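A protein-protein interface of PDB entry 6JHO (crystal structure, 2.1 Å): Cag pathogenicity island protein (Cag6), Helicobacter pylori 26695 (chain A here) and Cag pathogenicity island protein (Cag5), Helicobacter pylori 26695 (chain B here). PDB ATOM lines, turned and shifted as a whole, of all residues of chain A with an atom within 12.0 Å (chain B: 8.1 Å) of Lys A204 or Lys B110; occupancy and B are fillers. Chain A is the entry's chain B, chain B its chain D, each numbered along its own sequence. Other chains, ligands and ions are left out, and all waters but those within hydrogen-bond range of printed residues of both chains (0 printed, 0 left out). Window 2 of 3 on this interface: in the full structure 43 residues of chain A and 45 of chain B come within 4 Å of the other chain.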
ATOM      1  N   LEU A 191     -25.192  17.266  19.969  1.00  0.00           N
ATOM      2  CA  LEU A 191     -25.642  17.000  21.328  1.00  0.00           C
ATOM      3  C   LEU A 191     -25.029  17.974  22.326  1.00  0.00           C
ATOM      4  O   LEU A 191     -23.908  18.463  22.156  1.00  0.00           O
ATOM      5  CB  LEU A 191     -25.268  15.577  21.732  1.00  0.00           C
ATOM      6  CG  LEU A 191     -25.830  14.488  20.833  1.00  0.00           C
ATOM      7  CD1 LEU A 191     -24.996  13.250  21.000  1.00  0.00           C
ATOM      8  CD2 LEU A 191     -27.305  14.230  21.168  1.00  0.00           C
ATOM      9  N   GLU A 195     -26.481  15.325  27.211  1.00  0.00           N
ATOM     10  CA  GLU A 195     -27.176  14.386  26.332  1.00  0.00           C
ATOM     11  C   GLU A 195     -26.212  13.356  25.765  1.00  0.00           C
ATOM     12  O   GLU A 195     -26.574  12.189  25.572  1.00  0.00           O
ATOM     13  CB  GLU A 195     -27.873  15.110  25.174  1.00  0.00           C
ATOM     14  CG  GLU A 195     -28.977  16.097  25.563  1.00  0.00           C
ATOM     15  CD  GLU A 195     -29.369  17.009  24.402  1.00  0.00           C
ATOM     16  OE1 GLU A 195     -28.595  17.129  23.409  1.00  0.00           O
ATOM     17  OE2 GLU A 195     -30.462  17.608  24.484  1.00  0.00           O
ATOM     18  N   ARG A 196     -24.984  13.776  25.465  1.00  0.00           N
ATOM     19  CA  ARG A 196     -24.043  12.851  24.848  1.00  0.00           C
ATOM     20  C   ARG A 196     -23.567  11.804  25.853  1.00  0.00           C
ATOM     21  O   ARG A 196     -23.495  10.611  25.531  1.00  0.00           O
ATOM     22  CB  ARG A 196     -22.869  13.621  24.264  1.00  0.00           C
ATOM     23  CG  ARG A 196     -21.796  12.739  23.656  1.00  0.00           C
ATOM     24  CD  ARG A 196     -20.664  13.636  23.206  1.00  0.00           C
ATOM     25  NE  ARG A 196     -19.573  12.955  22.514  1.00  0.00           N
ATOM     26  CZ  ARG A 196     -18.362  12.828  23.039  1.00  0.00           C
ATOM     27  NH1 ARG A 196     -18.129  13.286  24.265  1.00  0.00           N
ATOM     28  NH2 ARG A 196     -17.400  12.234  22.357  1.00  0.00           N
ATOM     29  N   ALA A 197     -23.243  12.231  27.074  1.00  0.00           N
ATOM     30  CA  ALA A 197     -22.858  11.271  28.103  1.00  0.00           C
ATOM     31  C   ALA A 197     -23.991  10.287  28.380  1.00  0.00           C
ATOM     32  O   ALA A 197     -23.750   9.091  28.582  1.00  0.00           O
ATOM     33  CB  ALA A 197     -22.442  12.006  29.376  1.00  0.00           C
ATOM     34  N   LYS A 198     -25.237  10.765  28.350  1.00  0.00           N
ATOM     35  CA  LYS A 198     -26.384   9.875  28.507  1.00  0.00           C
ATOM     36  C   LYS A 198     -26.466   8.865  27.365  1.00  0.00           C
ATOM     37  O   LYS A 198     -26.632   7.661  27.595  1.00  0.00           O
ATOM     38  CB  LYS A 198     -27.674  10.692  28.579  1.00  0.00           C
ATOM     39  CG  LYS A 198     -28.321  10.764  29.954  1.00  0.00           C
ATOM     40  CD  LYS A 198     -29.469  11.785  29.977  1.00  0.00           C
ATOM     41  CE  LYS A 198     -30.160  11.820  31.340  1.00  0.00           C
ATOM     42  NZ  LYS A 198     -30.895  13.101  31.555  1.00  0.00           N
ATOM     43  N   LEU A 199     -26.374   9.341  26.117  1.00  0.00           N
ATOM     44  CA  LEU A 199     -26.503   8.429  24.985  1.00  0.00           C
ATOM     45  C   LEU A 199     -25.373   7.410  24.954  1.00  0.00           C
ATOM     46  O   LEU A 199     -25.569   6.276  24.506  1.00  0.00           O
ATOM     47  CB  LEU A 199     -26.534   9.211  23.674  1.00  0.00           C
ATOM     48  CG  LEU A 199     -26.851   8.377  22.438  1.00  0.00           C
ATOM     49  CD1 LEU A 199     -28.196   7.677  22.594  1.00  0.00           C
ATOM     50  CD2 LEU A 199     -26.848   9.253  21.203  1.00  0.00           C
ATOM     51  N   ILE A 200     -24.179   7.801  25.390  1.00  0.00           N
ATOM     52  CA  ILE A 200     -23.055   6.870  25.422  1.00  0.00           C
ATOM     53  C   ILE A 200     -23.337   5.744  26.413  1.00  0.00           C
ATOM     54  O   ILE A 200     -23.109   4.563  26.119  1.00  0.00           O
ATOM     55  CB  ILE A 200     -21.756   7.631  25.760  1.00  0.00           C
ATOM     56  CG1 ILE A 200     -21.279   8.445  24.542  1.00  0.00           C
ATOM     57  CG2 ILE A 200     -20.674   6.671  26.257  1.00  0.00           C
ATOM     58  CD1 ILE A 200     -20.187   9.414  24.852  1.00  0.00           C
ATOM     59  N   THR A 201     -23.849   6.098  27.598  1.00  0.00           N
ATOM     60  CA  THR A 201     -24.286   5.108  28.580  1.00  0.00           C
ATOM     61  C   THR A 201     -25.345   4.186  27.990  1.00  0.00           C
ATOM     62  O   THR A 201     -25.160   2.967  27.915  1.00  0.00           O
ATOM     63  CB  THR A 201     -24.830   5.823  29.817  1.00  0.00           C
ATOM     64  OG1 THR A 201     -23.818   6.688  30.350  1.00  0.00           O
ATOM     65  CG2 THR A 201     -25.258   4.821  30.882  1.00  0.00           C
ATOM     66  N   GLN A 202     -26.456   4.769  27.540  1.00  0.00           N
ATOM     67  CA  GLN A 202     -27.551   3.997  26.960  1.00  0.00           C
ATOM     68  C   GLN A 202     -27.072   3.043  25.869  1.00  0.00           C
ATOM     69  O   GLN A 202     -27.591   1.930  25.733  1.00  0.00           O
ATOM     70  CB  GLN A 202     -28.604   4.955  26.406  1.00  0.00           C
ATOM     71  CG  GLN A 202     -29.680   4.293  25.566  1.00  0.00           C
ATOM     72  CD  GLN A 202     -30.351   5.266  24.594  1.00  0.00           C
ATOM     73  OE1 GLN A 202     -30.709   6.391  24.964  1.00  0.00           O
ATOM     74  NE2 GLN A 202     -30.530   4.830  23.343  1.00  0.00           N
ATOM     75  N   LEU A 203     -26.090   3.462  25.072  1.00  0.00           N
ATOM     76  CA  LEU A 203     -25.599   2.629  23.983  1.00  0.00           C
ATOM     77  C   LEU A 203     -24.538   1.640  24.436  1.00  0.00           C
ATOM     78  O   LEU A 203     -24.103   0.811  23.630  1.00  0.00           O
ATOM     79  CB  LEU A 203     -25.023   3.506  22.867  1.00  0.00           C
ATOM     80  CG  LEU A 203     -25.992   4.269  21.964  1.00  0.00           C
ATOM     81  CD1 LEU A 203     -25.217   5.249  21.039  1.00  0.00           C
ATOM     82  CD2 LEU A 203     -26.840   3.304  21.154  1.00  0.00           C
ATOM     83  N   LYS A 204     -24.106   1.719  25.690  1.00  0.00           N
ATOM     84  CA  LYS A 204     -23.033   0.877  26.205  1.00  0.00           C
ATOM     85  C   LYS A 204     -21.799   0.950  25.310  1.00  0.00           C
ATOM     86  O   LYS A 204     -21.119  -0.048  25.066  1.00  0.00           O
ATOM     87  CB  LYS A 204     -23.498  -0.573  26.382  1.00  0.00           C
ATOM     88  CG  LYS A 204     -24.769  -0.743  27.214  1.00  0.00           C
ATOM     89  CD  LYS A 204     -25.099  -2.228  27.423  1.00  0.00           C
ATOM     90  CE  LYS A 204     -26.459  -2.418  28.072  1.00  0.00           C
ATOM     91  NZ  LYS A 204     -27.020  -1.108  28.530  1.00  0.00           N
ATOM     92  N   LEU A 205     -21.516   2.142  24.792  1.00  0.00           N
ATOM     93  CA  LEU A 205     -20.218   2.403  24.194  1.00  0.00           C
ATOM     94  C   LEU A 205     -19.199   2.588  25.305  1.00  0.00           C
ATOM     95  O   LEU A 205     -19.417   3.370  26.236  1.00  0.00           O
ATOM     96  CB  LEU A 205     -20.256   3.655  23.313  1.00  0.00           C
ATOM     97  CG  LEU A 205     -21.074   3.643  22.021  1.00  0.00           C
ATOM     98  CD1 LEU A 205     -21.180   5.060  21.488  1.00  0.00           C
ATOM     99  CD2 LEU A 205     -20.433   2.728  20.994  1.00  0.00           C
ATOM    100  N   ASN A 206     -18.089   1.879  25.218  1.00  0.00           N
ATOM    101  CA  ASN A 206     -16.988   2.104  26.143  1.00  0.00           C
ATOM    102  C   ASN A 206     -15.878   2.744  25.321  1.00  0.00           C
ATOM    103  O   ASN A 206     -15.226   2.077  24.513  1.00  0.00           O
ATOM    104  CB  ASN A 206     -16.547   0.805  26.821  1.00  0.00           C
ATOM    105  CG  ASN A 206     -15.216   0.949  27.544  1.00  0.00           C
ATOM    106  OD1 ASN A 206     -14.235   0.271  27.211  1.00  0.00           O
ATOM    107  ND2 ASN A 206     -15.169   1.852  28.525  1.00  0.00           N
ATOM    108  N   LEU A 207     -15.682   4.041  25.516  1.00  0.00           N
ATOM    109  CA  LEU A 207     -14.785   4.828  24.691  1.00  0.00           C
ATOM    110  C   LEU A 207     -13.423   4.951  25.362  1.00  0.00           C
ATOM    111  O   LEU A 207     -13.329   5.087  26.588  1.00  0.00           O
ATOM    112  CB  LEU A 207     -15.384   6.214  24.420  1.00  0.00           C
ATOM    113  CG  LEU A 207     -16.769   6.149  23.758  1.00  0.00           C
ATOM    114  CD1 LEU A 207     -17.401   7.521  23.628  1.00  0.00           C
ATOM    115  CD2 LEU A 207     -16.700   5.476  22.399  1.00  0.00           C
ATOM    116  N   GLU A 208     -12.375   4.881  24.536  1.00  0.00           N
ATOM    117  CA  GLU A 208     -10.968   4.989  24.937  1.00  0.00           C
ATOM    118  C   GLU A 208     -10.488   3.756  25.698  1.00  0.00           C
ATOM    119  O   GLU A 208      -9.832   2.878  25.125  1.00  0.00           O
ATOM    120  CB  GLU A 208     -10.742   6.244  25.772  1.00  0.00           C
ATOM    121  CG  GLU A 208     -11.149   7.527  25.070  1.00  0.00           C
ATOM    122  CD  GLU A 208     -10.809   8.730  25.895  1.00  0.00           C
ATOM    123  OE1 GLU A 208     -10.511   8.512  27.092  1.00  0.00           O
ATOM    124  OE2 GLU A 208     -10.824   9.873  25.364  1.00  0.00           O
ATOM    125  N   LEU B  99     -19.690  11.891  13.845  1.00  0.00           N
ATOM    126  CA  LEU B  99     -19.909  10.538  14.355  1.00  0.00           C
ATOM    127  C   LEU B  99     -20.071  10.523  15.865  1.00  0.00           C
ATOM    128  O   LEU B  99     -20.846   9.726  16.394  1.00  0.00           O
ATOM    129  CB  LEU B  99     -18.749   9.607  13.974  1.00  0.00           C
ATOM    130  CG  LEU B  99     -18.506   9.366  12.478  1.00  0.00           C
ATOM    131  CD1 LEU B  99     -17.508   8.235  12.283  1.00  0.00           C
ATOM    132  CD2 LEU B  99     -19.785   9.115  11.723  1.00  0.00           C
ATOM    133  N   MET B 100     -19.338  11.375  16.578  1.00  0.00           N
ATOM    134  CA  MET B 100     -19.260  11.264  18.022  1.00  0.00           C
ATOM    135  C   MET B 100     -20.081  12.317  18.766  1.00  0.00           C
ATOM    136  O   MET B 100     -20.224  12.213  19.989  1.00  0.00           O
ATOM    137  CB  MET B 100     -17.790  11.325  18.468  1.00  0.00           C
ATOM    138  CG  MET B 100     -16.943  10.244  17.821  1.00  0.00           C
ATOM    139  SD  MET B 100     -17.517   8.577  18.315  1.00  0.00           S
ATOM    140  CE  MET B 100     -17.056   8.623  20.042  1.00  0.00           C
ATOM    141  N   LYS B 103     -26.643  12.245  17.647  1.00  0.00           N
ATOM    142  CA  LYS B 103     -27.339  11.012  18.010  1.00  0.00           C
ATOM    143  C   LYS B 103     -27.192   9.958  16.920  1.00  0.00           C
ATOM    144  O   LYS B 103     -26.785   8.820  17.187  1.00  0.00           O
ATOM    145  CB  LYS B 103     -28.813  11.312  18.278  1.00  0.00           C
ATOM    146  CG  LYS B 103     -29.649  10.090  18.663  1.00  0.00           C
ATOM    147  CD  LYS B 103     -31.072  10.530  19.013  1.00  0.00           C
ATOM    148  CE  LYS B 103     -31.832   9.433  19.729  1.00  0.00           C
ATOM    149  NZ  LYS B 103     -32.539   8.606  18.738  1.00  0.00           N
ATOM    150  N   LYS B 104     -27.511  10.319  15.675  1.00  0.00           N
ATOM    151  CA  LYS B 104     -27.420   9.330  14.609  1.00  0.00           C
ATOM    152  C   LYS B 104     -25.976   8.916  14.357  1.00  0.00           C
ATOM    153  O   LYS B 104     -25.727   7.762  13.986  1.00  0.00           O
ATOM    154  CB  LYS B 104     -28.084   9.851  13.334  1.00  0.00           C
ATOM    155  CG  LYS B 104     -27.207  10.700  12.459  1.00  0.00           C
ATOM    156  CD  LYS B 104     -27.735  10.736  11.040  1.00  0.00           C
ATOM    157  CE  LYS B 104     -27.259  11.975  10.312  1.00  0.00           C
ATOM    158  NZ  LYS B 104     -28.204  12.354   9.223  1.00  0.00           N
ATOM    159  N   GLY B 105     -25.017   9.816  14.604  1.00  0.00           N
ATOM    160  CA  GLY B 105     -23.617   9.430  14.509  1.00  0.00           C
ATOM    161  C   GLY B 105     -23.228   8.390  15.547  1.00  0.00           C
ATOM    162  O   GLY B 105     -22.589   7.384  15.231  1.00  0.00           O
ATOM    163  N   LEU B 106     -23.585   8.630  16.810  1.00  0.00           N
ATOM    164  CA  LEU B 106     -23.202   7.691  17.862  1.00  0.00           C
ATOM    165  C   LEU B 106     -23.915   6.349  17.705  1.00  0.00           C
ATOM    166  O   LEU B 106     -23.324   5.305  18.001  1.00  0.00           O
ATOM    167  CB  LEU B 106     -23.480   8.294  19.235  1.00  0.00           C
ATOM    168  CG  LEU B 106     -22.435   9.303  19.738  1.00  0.00           C
ATOM    169  CD1 LEU B 106     -22.943  10.022  20.967  1.00  0.00           C
ATOM    170  CD2 LEU B 106     -21.067   8.640  20.017  1.00  0.00           C
ATOM    171  N   GLU B 107     -25.155   6.347  17.211  1.00  0.00           N
ATOM    172  CA  GLU B 107     -25.818   5.079  16.909  1.00  0.00           C
ATOM    173  C   GLU B 107     -25.095   4.345  15.793  1.00  0.00           C
ATOM    174  O   GLU B 107     -24.946   3.121  15.839  1.00  0.00           O
ATOM    175  CB  GLU B 107     -27.282   5.305  16.518  1.00  0.00           C
ATOM    176  CG  GLU B 107     -28.163   5.780  17.678  1.00  0.00           C
ATOM    177  CD  GLU B 107     -29.512   6.265  17.205  1.00  0.00           C
ATOM    178  OE1 GLU B 107     -29.786   6.167  15.994  1.00  0.00           O
ATOM    179  OE2 GLU B 107     -30.312   6.733  18.045  1.00  0.00           O
ATOM    180  N   PHE B 108     -24.646   5.088  14.777  1.00  0.00           N
ATOM    181  CA  PHE B 108     -23.870   4.505  13.687  1.00  0.00           C
ATOM    182  C   PHE B 108     -22.546   3.949  14.186  1.00  0.00           C
ATOM    183  O   PHE B 108     -22.100   2.890  13.736  1.00  0.00           O
ATOM    184  CB  PHE B 108     -23.650   5.575  12.619  1.00  0.00           C
ATOM    185  CG  PHE B 108     -22.736   5.167  11.494  1.00  0.00           C
ATOM    186  CD1 PHE B 108     -23.237   4.512  10.378  1.00  0.00           C
ATOM    187  CD2 PHE B 108     -21.390   5.493  11.523  1.00  0.00           C
ATOM    188  CE1 PHE B 108     -22.416   4.168   9.331  1.00  0.00           C
ATOM    189  CE2 PHE B 108     -20.560   5.154  10.466  1.00  0.00           C
ATOM    190  CZ  PHE B 108     -21.075   4.489   9.372  1.00  0.00           C
ATOM    191  N   VAL B 109     -21.898   4.655  15.115  1.00  0.00           N
ATOM    192  CA  VAL B 109     -20.631   4.189  15.675  1.00  0.00           C
ATOM    193  C   VAL B 109     -20.829   2.888  16.453  1.00  0.00           C
ATOM    194  O   VAL B 109     -19.996   1.971  16.394  1.00  0.00           O
ATOM    195  CB  VAL B 109     -20.016   5.290  16.557  1.00  0.00           C
ATOM    196  CG1 VAL B 109     -18.914   4.716  17.430  1.00  0.00           C
ATOM    197  CG2 VAL B 109     -19.496   6.460  15.685  1.00  0.00           C
ATOM    198  N   LYS B 110     -21.928   2.791  17.200  1.00  0.00           N
ATOM    199  CA  LYS B 110     -22.244   1.548  17.899  1.00  0.00           C
ATOM    200  C   LYS B 110     -22.471   0.412  16.906  1.00  0.00           C
ATOM    201  O   LYS B 110     -21.823  -0.636  16.992  1.00  0.00           O
ATOM    202  CB  LYS B 110     -23.468   1.746  18.793  1.00  0.00           C
ATOM    203  CG  LYS B 110     -23.930   0.471  19.503  1.00  0.00           C
ATOM    204  CD  LYS B 110     -22.979   0.114  20.625  1.00  0.00           C
ATOM    205  CE  LYS B 110     -23.422  -1.160  21.370  1.00  0.00           C
ATOM    206  NZ  LYS B 110     -22.507  -1.414  22.536  1.00  0.00           N
ATOM    207  N   ARG B 111     -23.340   0.634  15.919  1.00  0.00           N
ATOM    208  CA  ARG B 111     -23.690  -0.413  14.963  1.00  0.00           C
ATOM    209  C   ARG B 111     -22.471  -0.924  14.193  1.00  0.00           C
ATOM    210  O   ARG B 111     -22.299  -2.137  14.023  1.00  0.00           O
ATOM    211  CB  ARG B 111     -24.738   0.117  13.994  1.00  0.00           C
ATOM    212  CG  ARG B 111     -26.164  -0.090  14.444  1.00  0.00           C
ATOM    213  CD  ARG B 111     -27.127   0.577  13.472  1.00  0.00           C
ATOM    214  NE  ARG B 111     -26.485   0.841  12.185  1.00  0.00           N
ATOM    215  CZ  ARG B 111     -26.455   2.030  11.574  1.00  0.00           C
ATOM    216  NH1 ARG B 111     -27.047   3.097  12.121  1.00  0.00           N
ATOM    217  NH2 ARG B 111     -25.830   2.150  10.398  1.00  0.00           N
ATOM    218  N   LYS B 112     -21.635  -0.015  13.680  1.00  0.00           N
ATOM    219  CA  LYS B 112     -20.477  -0.419  12.890  1.00  0.00           C
ATOM    220  C   LYS B 112     -19.268  -0.759  13.746  1.00  0.00           C
ATOM    221  O   LYS B 112     -18.230  -1.127  13.194  1.00  0.00           O
ATOM    222  CB  LYS B 112     -20.089   0.677  11.890  1.00  0.00           C
ATOM    223  CG  LYS B 112     -21.237   1.245  11.053  1.00  0.00           C
ATOM    224  CD  LYS B 112     -21.653   0.323   9.908  1.00  0.00           C
ATOM    225  CE  LYS B 112     -20.605   0.255   8.802  1.00  0.00           C
ATOM    226  NZ  LYS B 112     -21.124  -0.521   7.635  1.00  0.00           N
ATOM    227  N   LYS B 113     -19.374  -0.631  15.070  1.00  0.00           N
ATOM    228  CA  LYS B 113     -18.271  -0.909  15.995  1.00  0.00           C
ATOM    229  C   LYS B 113     -17.053  -0.042  15.676  1.00  0.00           C
ATOM    230  O   LYS B 113     -15.913  -0.513  15.684  1.00  0.00           O
ATOM    231  CB  LYS B 113     -17.888  -2.396  15.991  1.00  0.00           C
ATOM    232  CG  LYS B 113     -19.040  -3.348  16.255  1.00  0.00           C
ATOM    233  CD  LYS B 113     -18.628  -4.801  15.955  1.00  0.00           C
ATOM    234  CE  LYS B 113     -19.788  -5.763  16.165  1.00  0.00           C
ATOM    235  NZ  LYS B 113     -19.606  -6.586  17.395  1.00  0.00           N
ATOM    236  N   ILE B 114     -17.298   1.232  15.375  1.00  0.00           N
ATOM    237  CA  ILE B 114     -16.197   2.143  15.109  1.00  0.00           C
ATOM    238  C   ILE B 114     -15.504   2.474  16.423  1.00  0.00           C
ATOM    239  O   ILE B 114     -16.144   2.563  17.476  1.00  0.00           O
ATOM    240  CB  ILE B 114     -16.729   3.392  14.387  1.00  0.00           C
ATOM    241  CG1 ILE B 114     -17.163   3.014  12.973  1.00  0.00           C
ATOM    242  CG2 ILE B 114     -15.706   4.504  14.388  1.00  0.00           C
ATOM    243  CD1 ILE B 114     -17.811   4.115  12.213  1.00  0.00           C
ATOM    244  N   ILE B 115     -14.186   2.620  16.380  1.00  0.00           N
ATOM    245  CA  ILE B 115     -13.397   2.917  17.568  1.00  0.00           C
ATOM    246  C   ILE B 115     -12.862   4.341  17.456  1.00  0.00           C
ATOM    247  O   ILE B 115     -11.979   4.626  16.636  1.00  0.00           O
ATOM    248  CB  ILE B 115     -12.258   1.907  17.752  1.00  0.00           C
ATOM    249  CG1 ILE B 115     -12.835   0.490  17.884  1.00  0.00           C
ATOM    250  CG2 ILE B 115     -11.393   2.310  18.946  1.00  0.00           C
ATOM    251  CD1 ILE B 115     -11.951  -0.580  17.326  1.00  0.00           C
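N of Leu B106 sits at hydrogen-bond distance from O of Leu B99 (3.0 Å).
NZ of Lys B103 is in salt-bridge range of OE2 of Glu B107, at 3.0 Å.
O of Ile A200 sits at hydrogen-bond distance from N of Leu A205.
The side-chain amino group (NZ) of Lys B110 lies within hydrogen-bond range of the backbone carbonyl oxygen (O) of Lys A204, at 3.2 Å.
O of Met B100 sits at hydrogen-bond distance from NE of Arg A196, 2.7 Å away.
NZ of Lys B110 lies within hydrogen-bond range of O of Leu A203 (2.9 Å).
N of Lys B103 touches CD1 of Leu A191 (3.9 Å).
CD1 of Leu A191 touches CD1 of Leu B106, 3.8 Å away.
CG of Arg A196 touches CD1 of Leu B106 (3.99 Å).
Leu A199 touches Lys B103.
CD1 of Leu B106 touches CD2 of Leu A199 (3.99 Å).
Leu A203 touches Leu B106 (CD1 to O, 3.6 Å).
Leu A203 touches Glu B107.
Leu A205 touches Leu B106 (CD1 to CD2, 3.9 Å).
CD2 of Leu A205 touches CD of Lys B110, at 3.7 Å.
Met B100 touches Leu A207.
Lys A204 touches just one residue of chain B: Lys B110 (3.2 Å).
Printed residues of chain A within 4 Å of Lys B110: Leu A203 (2.9 Å), Lys A204 (3.2 Å) and Leu A205 (3.7 Å).
No residue of chain A comes within 4 Å of Val B109.
No residue of chain A comes within 4 Å of Arg B111.
No residue of chain A comes within 4 Å of Ile B114.
Printed residues of chain B within 4 Å of Leu A203: Leu B106, Glu B107 and Lys B110.
Printed residues of chain A within 4 Å of Leu B106: Leu A191 (3.8 Å), Arg A196 (3.99 Å), Leu A199 (3.99 Å), Leu A203 (3.6 Å) and Leu A205 (3.9 Å).
Phe B108 touches none of the printed residues of chain A.
The nearest printed residue of chain B that does not touch Leu A203 is Lys B103 (5.5 Å).
Of the 15 printed residues of chain A, 7 touch a printed residue of chain B.
Printed residues of chain A that touch a printed residue of chain B: Leu A191, Arg A196, Leu A199, Leu A203, Lys A204, Leu A205 and Leu A207.
Hydrophobic or aromatic side chains of chain A within 4 Å of the printed part of chain B: Leu A191, Leu A199, Leu A203, Leu A205 and Leu A207.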
